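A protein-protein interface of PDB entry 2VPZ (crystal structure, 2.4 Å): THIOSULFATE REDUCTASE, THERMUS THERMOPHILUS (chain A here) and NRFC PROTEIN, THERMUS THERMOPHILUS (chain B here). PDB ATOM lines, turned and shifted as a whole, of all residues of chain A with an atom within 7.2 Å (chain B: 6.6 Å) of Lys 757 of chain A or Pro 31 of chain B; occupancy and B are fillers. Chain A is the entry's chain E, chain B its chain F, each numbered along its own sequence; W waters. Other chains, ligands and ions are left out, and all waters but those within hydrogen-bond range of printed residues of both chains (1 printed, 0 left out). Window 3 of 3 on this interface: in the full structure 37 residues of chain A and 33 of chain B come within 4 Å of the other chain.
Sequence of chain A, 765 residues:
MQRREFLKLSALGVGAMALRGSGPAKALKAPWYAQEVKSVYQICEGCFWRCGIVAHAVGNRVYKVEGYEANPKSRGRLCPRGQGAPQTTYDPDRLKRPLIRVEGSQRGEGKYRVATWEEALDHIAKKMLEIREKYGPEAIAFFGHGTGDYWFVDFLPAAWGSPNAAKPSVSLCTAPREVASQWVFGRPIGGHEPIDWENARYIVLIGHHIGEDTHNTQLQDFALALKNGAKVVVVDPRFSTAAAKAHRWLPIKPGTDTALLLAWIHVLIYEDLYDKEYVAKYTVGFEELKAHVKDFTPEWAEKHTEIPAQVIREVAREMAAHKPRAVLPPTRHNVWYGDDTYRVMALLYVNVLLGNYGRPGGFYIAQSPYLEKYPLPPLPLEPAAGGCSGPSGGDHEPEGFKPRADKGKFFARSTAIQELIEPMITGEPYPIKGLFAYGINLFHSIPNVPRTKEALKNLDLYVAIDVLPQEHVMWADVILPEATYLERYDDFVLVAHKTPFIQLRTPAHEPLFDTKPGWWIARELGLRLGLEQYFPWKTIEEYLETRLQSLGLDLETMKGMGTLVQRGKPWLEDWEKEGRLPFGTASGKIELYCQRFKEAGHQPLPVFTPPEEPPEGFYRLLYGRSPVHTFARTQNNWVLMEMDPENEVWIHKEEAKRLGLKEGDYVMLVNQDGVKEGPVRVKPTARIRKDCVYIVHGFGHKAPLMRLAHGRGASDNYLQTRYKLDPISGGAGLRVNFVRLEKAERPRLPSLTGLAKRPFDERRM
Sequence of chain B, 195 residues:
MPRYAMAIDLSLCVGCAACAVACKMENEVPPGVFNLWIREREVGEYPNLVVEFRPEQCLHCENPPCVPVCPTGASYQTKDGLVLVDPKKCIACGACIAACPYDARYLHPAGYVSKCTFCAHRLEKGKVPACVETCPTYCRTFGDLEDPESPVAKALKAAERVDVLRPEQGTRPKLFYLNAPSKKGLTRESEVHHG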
ATOM      1  N   PRO A  92     -30.878  22.585  11.688  1.00  0.00           N
ATOM      2  CA  PRO A  92     -31.661  23.243  10.629  1.00  0.00           C
ATOM      3  C   PRO A  92     -31.380  22.167   9.510  1.00  0.00           C
ATOM      4  O   PRO A  92     -31.925  21.077   9.590  1.00  0.00           O
ATOM      5  CB  PRO A  92     -30.929  24.579  10.410  1.00  0.00           C
ATOM      6  CG  PRO A  92     -30.457  24.949  11.832  1.00  0.00           C
ATOM      7  CD  PRO A  92     -30.065  23.562  12.442  1.00  0.00           C
ATOM      8  N   TRP A 638     -23.538  20.220  15.763  1.00  0.00           N
ATOM      9  CA  TRP A 638     -22.693  21.293  16.344  1.00  0.00           C
ATOM     10  C   TRP A 638     -22.143  20.960  17.741  1.00  0.00           C
ATOM     11  O   TRP A 638     -20.982  21.253  18.056  1.00  0.00           O
ATOM     12  CB  TRP A 638     -23.357  22.717  16.340  1.00  0.00           C
ATOM     13  CG  TRP A 638     -24.462  23.043  17.385  1.00  0.00           C
ATOM     14  CD1 TRP A 638     -25.816  23.019  17.163  1.00  0.00           C
ATOM     15  CD2 TRP A 638     -24.296  23.412  18.787  1.00  0.00           C
ATOM     16  NE1 TRP A 638     -26.494  23.342  18.322  1.00  0.00           N
ATOM     17  CE2 TRP A 638     -25.601  23.594  19.330  1.00  0.00           C
ATOM     18  CE3 TRP A 638     -23.185  23.619  19.630  1.00  0.00           C
ATOM     19  CZ2 TRP A 638     -25.828  23.948  20.684  1.00  0.00           C
ATOM     20  CZ3 TRP A 638     -23.418  23.981  21.014  1.00  0.00           C
ATOM     21  CH2 TRP A 638     -24.730  24.144  21.502  1.00  0.00           C
ATOM     22  N   GLU A 642     -17.959  20.671  17.757  1.00  0.00           N
ATOM     23  CA  GLU A 642     -17.321  21.652  18.646  1.00  0.00           C
ATOM     24  C   GLU A 642     -16.218  20.974  19.491  1.00  0.00           C
ATOM     25  O   GLU A 642     -15.198  21.590  19.844  1.00  0.00           O
ATOM     26  CB  GLU A 642     -18.371  22.272  19.543  1.00  0.00           C
ATOM     27  CG  GLU A 642     -18.300  23.766  19.693  1.00  0.00           C
ATOM     28  CD  GLU A 642     -19.241  24.290  20.768  1.00  0.00           C
ATOM     29  OE1 GLU A 642     -19.884  23.452  21.426  1.00  0.00           O
ATOM     30  OE2 GLU A 642     -19.318  25.513  20.945  1.00  0.00           O
ATOM     31  N   LEU A 708     -22.188  22.422   8.213  1.00  0.00           N
ATOM     32  CA  LEU A 708     -21.048  22.252   9.133  1.00  0.00           C
ATOM     33  C   LEU A 708     -20.064  21.162   8.642  1.00  0.00           C
ATOM     34  O   LEU A 708     -18.847  21.330   8.696  1.00  0.00           O
ATOM     35  CB  LEU A 708     -21.480  21.804  10.547  1.00  0.00           C
ATOM     36  CG  LEU A 708     -22.552  22.358  11.499  1.00  0.00           C
ATOM     37  CD1 LEU A 708     -21.830  22.694  12.806  1.00  0.00           C
ATOM     38  CD2 LEU A 708     -23.329  23.577  10.948  1.00  0.00           C
ATOM     39  N   LEU A 752     -17.467  27.885  12.469  1.00  0.00           N
ATOM     40  CA  LEU A 752     -18.286  26.812  12.972  1.00  0.00           C
ATOM     41  C   LEU A 752     -19.243  27.282  14.105  1.00  0.00           C
ATOM     42  O   LEU A 752     -20.365  26.781  14.245  1.00  0.00           O
ATOM     43  CB  LEU A 752     -17.340  25.724  13.423  1.00  0.00           C
ATOM     44  CG  LEU A 752     -17.781  24.307  13.209  1.00  0.00           C
ATOM     45  CD1 LEU A 752     -16.566  23.438  12.940  1.00  0.00           C
ATOM     46  CD2 LEU A 752     -18.538  23.856  14.431  1.00  0.00           C
ATOM     47  N   THR A 753     -18.807  28.247  14.905  1.00  0.00           N
ATOM     48  CA  THR A 753     -19.639  28.783  15.987  1.00  0.00           C
ATOM     49  C   THR A 753     -20.796  29.589  15.354  1.00  0.00           C
ATOM     50  O   THR A 753     -21.947  29.494  15.791  1.00  0.00           O
ATOM     51  CB  THR A 753     -18.828  29.703  16.996  1.00  0.00           C
ATOM     52  OG1 THR A 753     -17.676  29.025  17.478  1.00  0.00           O
ATOM     53  CG2 THR A 753     -19.727  30.119  18.197  1.00  0.00           C
ATOM     54  N   GLY A 754     -20.465  30.361  14.319  1.00  0.00           N
ATOM     55  CA  GLY A 754     -21.424  31.152  13.566  1.00  0.00           C
ATOM     56  C   GLY A 754     -22.492  30.254  12.958  1.00  0.00           C
ATOM     57  O   GLY A 754     -23.690  30.561  12.977  1.00  0.00           O
ATOM     58  N   LEU A 755     -22.072  29.126  12.403  1.00  0.00           N
ATOM     59  CA  LEU A 755     -23.018  28.160  11.874  1.00  0.00           C
ATOM     60  C   LEU A 755     -23.764  27.461  13.048  1.00  0.00           C
ATOM     61  O   LEU A 755     -24.963  27.198  12.940  1.00  0.00           O
ATOM     62  CB  LEU A 755     -22.326  27.120  10.952  1.00  0.00           C
ATOM     63  CG  LEU A 755     -21.974  27.628   9.535  1.00  0.00           C
ATOM     64  CD1 LEU A 755     -20.880  26.797   8.866  1.00  0.00           C
ATOM     65  CD2 LEU A 755     -23.240  27.631   8.670  1.00  0.00           C
ATOM     66  N   ALA A 756     -23.113  27.194  14.177  1.00  0.00           N
ATOM     67  CA  ALA A 756     -23.819  26.513  15.278  1.00  0.00           C
ATOM     68  C   ALA A 756     -24.986  27.306  15.869  1.00  0.00           C
ATOM     69  O   ALA A 756     -25.953  26.726  16.375  1.00  0.00           O
ATOM     70  CB  ALA A 756     -22.839  26.106  16.424  1.00  0.00           C
ATOM     71  N   LYS A 757     -24.899  28.626  15.760  1.00  0.00           N
ATOM     72  CA  LYS A 757     -25.884  29.576  16.302  1.00  0.00           C
ATOM     73  C   LYS A 757     -27.244  29.777  15.596  1.00  0.00           C
ATOM     74  O   LYS A 757     -28.213  30.228  16.239  1.00  0.00           O
ATOM     75  CB  LYS A 757     -25.186  30.907  16.576  1.00  0.00           C
ATOM     76  CG  LYS A 757     -24.307  30.831  17.812  1.00  0.00           C
ATOM     77  CD  LYS A 757     -23.379  32.016  17.957  1.00  0.00           C
ATOM     78  CE  LYS A 757     -22.631  31.940  19.286  1.00  0.00           C
ATOM     79  NZ  LYS A 757     -22.105  33.261  19.765  1.00  0.00           N
ATOM     80  N   ARG A 758     -27.308  29.463  14.298  1.00  0.00           N
ATOM     81  CA  ARG A 758     -28.554  29.500  13.531  1.00  0.00           C
ATOM     82  C   ARG A 758     -29.550  28.790  14.404  1.00  0.00           C
ATOM     83  O   ARG A 758     -29.318  27.640  14.781  1.00  0.00           O
ATOM     84  CB  ARG A 758     -28.468  28.675  12.256  1.00  0.00           C
ATOM     85  CG  ARG A 758     -27.606  29.239  11.203  1.00  0.00           C
ATOM     86  CD  ARG A 758     -26.656  28.178  10.725  1.00  0.00           C
ATOM     87  NE  ARG A 758     -27.153  27.420   9.591  1.00  0.00           N
ATOM     88  CZ  ARG A 758     -27.156  26.099   9.480  1.00  0.00           C
ATOM     89  NH1 ARG A 758     -26.691  25.346  10.460  1.00  0.00           N
ATOM     90  NH2 ARG A 758     -27.593  25.529   8.362  1.00  0.00           N
ATOM     91  N   PRO A 759     -30.681  29.444  14.721  1.00  0.00           N
ATOM     92  CA  PRO A 759     -31.715  28.844  15.565  1.00  0.00           C
ATOM     93  C   PRO A 759     -32.541  27.771  14.839  1.00  0.00           C
ATOM     94  O   PRO A 759     -32.731  27.838  13.615  1.00  0.00           O
ATOM     95  CB  PRO A 759     -32.585  30.033  16.002  1.00  0.00           C
ATOM     96  CG  PRO A 759     -31.896  31.288  15.413  1.00  0.00           C
ATOM     97  CD  PRO A 759     -31.091  30.767  14.251  1.00  0.00           C
ATOM     98  N   PHE A 760     -33.015  26.788  15.598  1.00  0.00           N
ATOM     99  CA  PHE A 760     -33.847  25.729  15.051  1.00  0.00           C
ATOM    100  C   PHE A 760     -35.312  26.163  14.996  1.00  0.00           C
ATOM    101  O   PHE A 760     -35.986  26.328  16.027  1.00  0.00           O
ATOM    102  CB  PHE A 760     -33.756  24.424  15.849  1.00  0.00           C
ATOM    103  CG  PHE A 760     -34.591  23.319  15.268  1.00  0.00           C
ATOM    104  CD1 PHE A 760     -34.331  22.854  13.978  1.00  0.00           C
ATOM    105  CD2 PHE A 760     -35.651  22.766  15.981  1.00  0.00           C
ATOM    106  CE1 PHE A 760     -35.127  21.865  13.389  1.00  0.00           C
ATOM    107  CE2 PHE A 760     -36.461  21.778  15.407  1.00  0.00           C
ATOM    108  CZ  PHE A 760     -36.191  21.323  14.106  1.00  0.00           C
ATOM    109  N   LYS B  24     -22.655  20.327  28.549  1.00  0.00           N
ATOM    110  CA  LYS B  24     -23.257  21.143  27.460  1.00  0.00           C
ATOM    111  C   LYS B  24     -24.771  20.964  27.218  1.00  0.00           C
ATOM    112  O   LYS B  24     -25.465  21.869  26.728  1.00  0.00           O
ATOM    113  CB  LYS B  24     -22.609  20.825  26.104  1.00  0.00           C
ATOM    114  CG  LYS B  24     -21.438  21.648  25.719  1.00  0.00           C
ATOM    115  CD  LYS B  24     -21.840  22.892  24.987  1.00  0.00           C
ATOM    116  CE  LYS B  24     -20.571  23.622  24.649  1.00  0.00           C
ATOM    117  NZ  LYS B  24     -20.795  24.864  23.882  1.00  0.00           N
ATOM    118  N   VAL B  29     -25.011  25.116  27.777  1.00  0.00           N
ATOM    119  CA  VAL B  29     -23.867  26.010  27.582  1.00  0.00           C
ATOM    120  C   VAL B  29     -23.879  26.284  26.053  1.00  0.00           C
ATOM    121  O   VAL B  29     -23.970  25.342  25.251  1.00  0.00           O
ATOM    122  CB  VAL B  29     -22.523  25.345  28.130  1.00  0.00           C
ATOM    123  CG1 VAL B  29     -21.345  26.339  28.070  1.00  0.00           C
ATOM    124  CG2 VAL B  29     -22.746  24.870  29.600  1.00  0.00           C
ATOM    125  N   PRO B  30     -23.837  27.579  25.642  1.00  0.00           N
ATOM    126  CA  PRO B  30     -23.854  28.119  24.267  1.00  0.00           C
ATOM    127  C   PRO B  30     -22.646  27.739  23.380  1.00  0.00           C
ATOM    128  O   PRO B  30     -21.608  27.394  23.938  1.00  0.00           O
ATOM    129  CB  PRO B  30     -23.920  29.645  24.480  1.00  0.00           C
ATOM    130  CG  PRO B  30     -24.063  29.837  26.050  1.00  0.00           C
ATOM    131  CD  PRO B  30     -23.383  28.614  26.572  1.00  0.00           C
ATOM    132  N   PRO B  31     -22.781  27.755  22.011  1.00  0.00           N
ATOM    133  CA  PRO B  31     -21.653  27.419  21.117  1.00  0.00           C
ATOM    134  C   PRO B  31     -20.398  28.326  21.331  1.00  0.00           C
ATOM    135  O   PRO B  31     -20.544  29.541  21.512  1.00  0.00           O
ATOM    136  CB  PRO B  31     -22.195  27.664  19.705  1.00  0.00           C
ATOM    137  CG  PRO B  31     -23.672  27.476  19.803  1.00  0.00           C
ATOM    138  CD  PRO B  31     -24.061  27.714  21.277  1.00  0.00           C
ATOM    139  N   GLY B  32     -19.190  27.762  21.280  1.00  0.00           N
ATOM    140  CA  GLY B  32     -17.970  28.535  21.419  1.00  0.00           C
ATOM    141  C   GLY B  32     -17.358  28.670  22.805  1.00  0.00           C
ATOM    142  O   GLY B  32     -16.221  29.127  22.961  1.00  0.00           O
ATOM    143  N   VAL B  33     -18.106  28.274  23.822  1.00  0.00           N
ATOM    144  CA  VAL B  33     -17.625  28.344  25.188  1.00  0.00           C
ATOM    145  C   VAL B  33     -17.899  27.021  25.941  1.00  0.00           C
ATOM    146  O   VAL B  33     -18.844  26.298  25.621  1.00  0.00           O
ATOM    147  CB  VAL B  33     -18.189  29.606  25.869  1.00  0.00           C
ATOM    148  CG1 VAL B  33     -17.700  30.848  25.095  1.00  0.00           C
ATOM    149  CG2 VAL B  33     -19.707  29.562  25.876  1.00  0.00           C
ATOM    150  N   PHE B  34     -17.063  26.728  26.930  1.00  0.00           N
ATOM    151  CA  PHE B  34     -17.081  25.454  27.642  1.00  0.00           C
ATOM    152  C   PHE B  34     -16.924  25.501  29.169  1.00  0.00           C
ATOM    153  O   PHE B  34     -16.020  26.160  29.658  1.00  0.00           O
ATOM    154  CB  PHE B  34     -15.923  24.588  27.054  1.00  0.00           C
ATOM    155  CG  PHE B  34     -15.984  24.358  25.539  1.00  0.00           C
ATOM    156  CD1 PHE B  34     -15.421  25.274  24.626  1.00  0.00           C
ATOM    157  CD2 PHE B  34     -16.661  23.243  25.030  1.00  0.00           C
ATOM    158  CE1 PHE B  34     -15.547  25.080  23.228  1.00  0.00           C
ATOM    159  CE2 PHE B  34     -16.798  23.024  23.651  1.00  0.00           C
ATOM    160  CZ  PHE B  34     -16.247  23.948  22.741  1.00  0.00           C
ATOM    161  N   PRO B 109     -23.070  34.982  26.068  1.00  0.00           N
ATOM    162  CA  PRO B 109     -23.642  35.894  25.059  1.00  0.00           C
ATOM    163  C   PRO B 109     -24.852  36.725  25.552  1.00  0.00           C
ATOM    164  O   PRO B 109     -25.376  37.584  24.836  1.00  0.00           O
ATOM    165  CB  PRO B 109     -24.002  34.991  23.871  1.00  0.00           C
ATOM    166  CG  PRO B 109     -23.829  33.552  24.383  1.00  0.00           C
ATOM    167  CD  PRO B 109     -22.793  33.665  25.488  1.00  0.00           C
HETATM  168  O   HOH W   1     -21.827  31.797  22.746  1.00  0.00           O
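The side-chain carboxylate (OE1) of Glu 642 of chain A is in salt-bridge range of the side-chain amino group (NZ) of Lys 24 of chain B (3.0 Å).
The side-chain carboxylate (OE2) of Glu 642 of chain A lies close to the backbone NH (N) of Gly 32 of chain B.
The backbone NH (N) of Val 29 of chain B is in hydrogen-bond range of the backbone carbonyl oxygen (O) of Lys 24 of chain B, at 3.4 Å.
The side-chain amino group of Lys 24 of chain B is in hydrogen-bond range of the backbone carbonyl oxygen of Pro 30 of chain B.
The side-chain amino group of Lys 24 of chain B is in hydrogen-bond range of the backbone carbonyl oxygen of Val 33 of chain B, at 3.0 Å.
Among the printed residues, merely in contact across the chains: Glu 642 of chain A with Pro 31 of chain B, Thr 753 of chain A with Pro 31 of chain B, Glu 642 of chain A with Phe 34 of chain B, Trp 638 of chain A with Pro 31 of chain B, Ala 756 of chain A with Pro 31 of chain B, Lys 757 of chain A with Pro 31 of chain B, Thr 753 of chain A with Gly 32 of chain B and Trp 638 of chain A with Lys 24 of chain B.
Of the printed residues of chain B, Glu 642 of chain A touches Lys 24, Pro 31, Gly 32 and Phe 34.
Leu 755 of chain A touches none of the printed residues of chain B.
Printed residues of chain B within 4 Å of Ala 756 of chain A: Pro 31.
Of chain B, only Pro 31 (3.9 Å) comes within 4 Å of Lys 757 of chain A.
Printed residues of chain A within 4 Å of Lys 24 of chain B: Trp 638 (3.99 Å) and Glu 642 (3.0 Å).
Printed residues of chain A within 4 Å of Pro 31 of chain B: Trp 638, Glu 642, Thr 753, Ala 756 and Lys 757.
The nearest residue of chain B that does not touch Lys 757 of chain A is Pro 109 of chain B (4.8 Å).
The nearest residue of chain A that does not touch Pro 31 of chain B is Leu 752 of chain A (5.8 Å).
Printed residues of chain B that touch a printed residue of chain A: Lys 24, Pro 31, Gly 32 and Phe 34.
Of the 13 printed residues of chain A, 5 touch a printed residue of chain B.
Printed residues of chain A that touch a printed residue of chain B: Trp 638, Glu 642, Thr 753, Ala 756 and Lys 757.
Along chain A the printed residues that touch a printed residue of chain B span positions 638 to 757.
Among the printed residues, Asp or Glu carboxylates within 4 Å of a Lys or Arg side-chain nitrogen of the other chain: Glu 642 of chain A with Lys 24 of chain B (3.0 Å).
Water W1 bridges the backbone carbonyl oxygen of Pro 31 of chain B and the side-chain amino group of Lys 757 of chain A.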
